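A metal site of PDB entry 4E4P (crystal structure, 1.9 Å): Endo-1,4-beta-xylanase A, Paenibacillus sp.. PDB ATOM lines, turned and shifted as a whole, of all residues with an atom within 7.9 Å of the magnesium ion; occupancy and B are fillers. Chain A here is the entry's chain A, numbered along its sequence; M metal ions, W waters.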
ATOM      1  N   TYR A  11      13.455 -23.721   4.698  1.00  0.00           N
ATOM      2  CA  TYR A  11      14.762 -23.558   5.355  1.00  0.00           C
ATOM      3  C   TYR A  11      16.017 -23.892   4.476  1.00  0.00           C
ATOM      4  O   TYR A  11      17.105 -24.170   5.000  1.00  0.00           O
ATOM      5  CB  TYR A  11      14.749 -24.299   6.700  1.00  0.00           C
ATOM      6  CG  TYR A  11      13.655 -23.733   7.603  1.00  0.00           C
ATOM      7  CD1 TYR A  11      13.712 -22.407   8.067  1.00  0.00           C
ATOM      8  CD2 TYR A  11      12.543 -24.506   7.987  1.00  0.00           C
ATOM      9  CE1 TYR A  11      12.712 -21.865   8.895  1.00  0.00           C
ATOM     10  CE2 TYR A  11      11.525 -23.963   8.829  1.00  0.00           C
ATOM     11  CZ  TYR A  11      11.625 -22.657   9.275  1.00  0.00           C
ATOM     12  OH  TYR A  11      10.648 -22.124  10.090  1.00  0.00           O
ATOM     13  N   LYS A  12      15.851 -23.799   3.154  1.00  0.00           N
ATOM     14  CA  LYS A  12      16.895 -24.144   2.157  1.00  0.00           C
ATOM     15  C   LYS A  12      18.282 -23.521   2.398  1.00  0.00           C
ATOM     16  O   LYS A  12      19.306 -24.200   2.325  1.00  0.00           O
ATOM     17  CB  LYS A  12      16.397 -23.813   0.728  1.00  0.00           C
ATOM     18  CG  LYS A  12      15.894 -22.360   0.510  1.00  0.00           C
ATOM     19  CD  LYS A  12      15.202 -22.142  -0.865  1.00  0.00           C
ATOM     20  CE  LYS A  12      14.339 -20.852  -0.931  1.00  0.00           C
ATOM     21  NZ  LYS A  12      13.274 -20.714   0.159  1.00  0.00           N
ATOM     22  N   ASN A  13      18.319 -22.223   2.673  1.00  0.00           N
ATOM     23  CA  ASN A  13      19.578 -21.537   2.931  1.00  0.00           C
ATOM     24  C   ASN A  13      20.035 -21.635   4.416  1.00  0.00           C
ATOM     25  O   ASN A  13      21.192 -21.328   4.744  1.00  0.00           O
ATOM     26  CB  ASN A  13      19.484 -20.078   2.441  1.00  0.00           C
ATOM     27  CG  ASN A  13      19.032 -19.971   0.976  1.00  0.00           C
ATOM     28  OD1 ASN A  13      19.449 -20.762   0.118  1.00  0.00           O
ATOM     29  ND2 ASN A  13      18.172 -18.993   0.684  1.00  0.00           N
ATOM     30  N   ASP A  14      19.133 -22.098   5.291  1.00  0.00           N
ATOM     31  CA  ASP A  14      19.301 -22.053   6.758  1.00  0.00           C
ATOM     32  C   ASP A  14      19.945 -23.366   7.328  1.00  0.00           C
ATOM     33  O   ASP A  14      21.000 -23.359   7.933  1.00  0.00           O
ATOM     34  CB  ASP A  14      17.932 -21.767   7.418  1.00  0.00           C
ATOM     35  CG  ASP A  14      17.292 -20.403   6.960  1.00  0.00           C
ATOM     36  OD1 ASP A  14      17.734 -19.305   7.407  1.00  0.00           O
ATOM     37  OD2 ASP A  14      16.301 -20.414   6.167  1.00  0.00           O
ATOM     38  N   PHE A  15      19.312 -24.497   7.121  1.00  0.00           N
ATOM     39  CA  PHE A  15      19.816 -25.744   7.701  1.00  0.00           C
ATOM     40  C   PHE A  15      19.122 -26.895   7.030  1.00  0.00           C
ATOM     41  O   PHE A  15      18.040 -26.738   6.486  1.00  0.00           O
ATOM     42  CB  PHE A  15      19.589 -25.836   9.258  1.00  0.00           C
ATOM     43  CG  PHE A  15      18.304 -25.192   9.752  1.00  0.00           C
ATOM     44  CD1 PHE A  15      17.079 -25.869   9.671  1.00  0.00           C
ATOM     45  CD2 PHE A  15      18.321 -23.933  10.352  1.00  0.00           C
ATOM     46  CE1 PHE A  15      15.885 -25.269  10.144  1.00  0.00           C
ATOM     47  CE2 PHE A  15      17.131 -23.316  10.821  1.00  0.00           C
ATOM     48  CZ  PHE A  15      15.904 -23.990  10.690  1.00  0.00           C
ATOM     49  N   LEU A  16      19.761 -28.051   7.079  1.00  0.00           N
ATOM     50  CA  LEU A  16      19.156 -29.280   6.574  1.00  0.00           C
ATOM     51  C   LEU A  16      17.940 -29.641   7.410  1.00  0.00           C
ATOM     52  O   LEU A  16      17.991 -29.470   8.587  1.00  0.00           O
ATOM     53  CB  LEU A  16      20.151 -30.427   6.695  1.00  0.00           C
ATOM     54  CG  LEU A  16      21.350 -30.267   5.740  1.00  0.00           C
ATOM     55  CD1 LEU A  16      22.317 -31.446   5.969  1.00  0.00           C
ATOM     56  CD2 LEU A  16      20.968 -30.096   4.283  1.00  0.00           C
ATOM     57  N   GLU A 257      29.748 -26.208  15.410  1.00  0.00           N
ATOM     58  CA  GLU A 257      28.391 -26.138  14.866  1.00  0.00           C
ATOM     59  C   GLU A 257      27.411 -26.822  15.814  1.00  0.00           C
ATOM     60  O   GLU A 257      27.787 -27.573  16.752  1.00  0.00           O
ATOM     61  CB  GLU A 257      28.354 -26.719  13.468  1.00  0.00           C
ATOM     62  CG  GLU A 257      28.651 -28.198  13.376  1.00  0.00           C
ATOM     63  CD  GLU A 257      28.477 -28.730  11.883  1.00  0.00           C
ATOM     64  OE1 GLU A 257      28.955 -28.026  10.929  1.00  0.00           O
ATOM     65  OE2 GLU A 257      27.848 -29.840  11.701  1.00  0.00           O
ATOM     66  N   VAL A 258      26.142 -26.536  15.630  1.00  0.00           N
ATOM     67  CA  VAL A 258      25.109 -27.081  16.486  1.00  0.00           C
ATOM     68  C   VAL A 258      24.047 -27.745  15.608  1.00  0.00           C
ATOM     69  O   VAL A 258      23.789 -27.275  14.494  1.00  0.00           O
ATOM     70  CB  VAL A 258      24.404 -25.996  17.325  1.00  0.00           C
ATOM     71  CG1 VAL A 258      23.091 -26.616  17.905  1.00  0.00           C
ATOM     72  CG2 VAL A 258      25.319 -25.602  18.490  1.00  0.00           C
ATOM     73  N   TYR A 292      15.890 -20.923  15.783  1.00  0.00           N
ATOM     74  CA  TYR A 292      16.839 -21.454  14.824  1.00  0.00           C
ATOM     75  C   TYR A 292      17.160 -20.547  13.674  1.00  0.00           C
ATOM     76  O   TYR A 292      18.324 -20.400  13.334  1.00  0.00           O
ATOM     77  CB  TYR A 292      16.383 -22.775  14.278  1.00  0.00           C
ATOM     78  CG  TYR A 292      16.059 -23.720  15.386  1.00  0.00           C
ATOM     79  CD1 TYR A 292      16.763 -23.680  16.558  1.00  0.00           C
ATOM     80  CD2 TYR A 292      15.080 -24.704  15.240  1.00  0.00           C
ATOM     81  CE1 TYR A 292      16.512 -24.575  17.583  1.00  0.00           C
ATOM     82  CE2 TYR A 292      14.833 -25.582  16.261  1.00  0.00           C
ATOM     83  CZ  TYR A 292      15.545 -25.511  17.413  1.00  0.00           C
ATOM     84  OH  TYR A 292      15.290 -26.369  18.438  1.00  0.00           O
ATOM     85  N   HIS A 295      19.716 -18.196  14.501  1.00  0.00           N
ATOM     86  CA  HIS A 295      21.093 -18.645  14.601  1.00  0.00           C
ATOM     87  C   HIS A 295      21.513 -19.590  13.493  1.00  0.00           C
ATOM     88  O   HIS A 295      22.415 -20.397  13.693  1.00  0.00           O
ATOM     89  CB  HIS A 295      21.301 -19.314  15.993  1.00  0.00           C
ATOM     90  CG  HIS A 295      21.236 -18.352  17.151  1.00  0.00           C
ATOM     91  ND1 HIS A 295      20.097 -18.166  17.908  1.00  0.00           N
ATOM     92  CD2 HIS A 295      22.155 -17.505  17.656  1.00  0.00           C
ATOM     93  CE1 HIS A 295      20.319 -17.246  18.832  1.00  0.00           C
ATOM     94  NE2 HIS A 295      21.559 -16.827  18.704  1.00  0.00           N
ATOM     95  N   ALA A 296      20.860 -19.512  12.340  1.00  0.00           N
ATOM     96  CA  ALA A 296      21.041 -20.504  11.258  1.00  0.00           C
ATOM     97  C   ALA A 296      22.483 -20.612  10.757  1.00  0.00           C
ATOM     98  O   ALA A 296      22.850 -21.620  10.145  1.00  0.00           O
ATOM     99  CB  ALA A 296      20.137 -20.139  10.094  1.00  0.00           C
ATOM    100  N   ASP A 297      23.270 -19.561  10.956  1.00  0.00           N
ATOM    101  CA  ASP A 297      24.687 -19.615  10.574  1.00  0.00           C
ATOM    102  C   ASP A 297      25.413 -20.702  11.365  1.00  0.00           C
ATOM    103  O   ASP A 297      26.468 -21.186  10.950  1.00  0.00           O
ATOM    104  CB  ASP A 297      25.383 -18.267  10.759  1.00  0.00           C
ATOM    105  CG  ASP A 297      25.093 -17.297   9.625  1.00  0.00           C
ATOM    106  OD1 ASP A 297      24.408 -16.268   9.848  1.00  0.00           O
ATOM    107  OD2 ASP A 297      25.576 -17.549   8.487  1.00  0.00           O
ATOM    108  N   HIS A 298      24.859 -21.132  12.481  1.00  0.00           N
ATOM    109  CA  HIS A 298      25.598 -22.043  13.352  1.00  0.00           C
ATOM    110  C   HIS A 298      24.967 -23.410  13.480  1.00  0.00           C
ATOM    111  O   HIS A 298      25.508 -24.285  14.123  1.00  0.00           O
ATOM    112  CB  HIS A 298      25.704 -21.457  14.734  1.00  0.00           C
ATOM    113  CG  HIS A 298      26.356 -20.131  14.729  1.00  0.00           C
ATOM    114  ND1 HIS A 298      27.697 -19.983  14.481  1.00  0.00           N
ATOM    115  CD2 HIS A 298      25.848 -18.882  14.905  1.00  0.00           C
ATOM    116  CE1 HIS A 298      28.006 -18.699  14.524  1.00  0.00           C
ATOM    117  NE2 HIS A 298      26.906 -18.014  14.777  1.00  0.00           N
ATOM    118  N   ILE A 299      23.825 -23.580  12.865  1.00  0.00           N
ATOM    119  CA  ILE A 299      23.056 -24.798  13.002  1.00  0.00           C
ATOM    120  C   ILE A 299      23.120 -25.556  11.623  1.00  0.00           C
ATOM    121  O   ILE A 299      22.713 -25.053  10.677  1.00  0.00           O
ATOM    122  CB  ILE A 299      21.580 -24.374  13.318  1.00  0.00           C
ATOM    123  CG1 ILE A 299      21.503 -23.807  14.750  1.00  0.00           C
ATOM    124  CG2 ILE A 299      20.634 -25.534  13.085  1.00  0.00           C
ATOM    125  CD1 ILE A 299      20.214 -23.244  15.195  1.00  0.00           C
ATOM    126  N   ALA A 300      23.579 -26.794  11.597  1.00  0.00           N
ATOM    127  CA  ALA A 300      23.756 -27.489  10.305  1.00  0.00           C
ATOM    128  C   ALA A 300      22.481 -28.248   9.881  1.00  0.00           C
ATOM    129  O   ALA A 300      22.121 -28.288   8.718  1.00  0.00           O
ATOM    130  CB  ALA A 300      24.970 -28.416  10.394  1.00  0.00           C
ATOM    131  N   ARG A 301      21.742 -28.720  10.871  1.00  0.00           N
ATOM    132  CA  ARG A 301      20.640 -29.658  10.689  1.00  0.00           C
ATOM    133  C   ARG A 301      19.624 -29.523  11.821  1.00  0.00           C
ATOM    134  O   ARG A 301      19.993 -29.446  12.991  1.00  0.00           O
ATOM    135  CB  ARG A 301      21.263 -31.087  10.742  1.00  0.00           C
ATOM    136  CG  ARG A 301      20.306 -32.280  10.753  1.00  0.00           C
ATOM    137  CD  ARG A 301      21.109 -33.602  10.501  1.00  0.00           C
ATOM    138  NE  ARG A 301      22.245 -33.650  11.440  1.00  0.00           N
ATOM    139  CZ  ARG A 301      22.163 -34.166  12.654  1.00  0.00           C
ATOM    140  NH1 ARG A 301      23.211 -34.140  13.465  1.00  0.00           N
ATOM    141  NH2 ARG A 301      20.998 -34.654  13.069  1.00  0.00           N
HETATM  142 MG    MG M   1      23.098 -23.560   8.999  1.00  0.00          MG
HETATM  143  O   HOH W   1      23.368 -22.082   7.353  1.00  0.00           O
HETATM  144  O   HOH W   2      25.367 -23.245   9.073  1.00  0.00           O
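Three residues have an atom within 4 Å of the magnesium ion: Asp 14, Ala 296 and Ile 299.
Along chain A the residues within 4 Å of the magnesium ion span positions 14 to 299.
The magnesium ion is bound by water W1 (2.2 Å), the backbone carbonyl oxygen of Ala 296 (2.3 Å), the backbone carbonyl oxygen of Ile 299 (2.3 Å), water W2 (2.3 Å) and the backbone carbonyl oxygen of Asp 14 (2.4 Å).
The magnesium ion has five donor atoms within binding distance.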
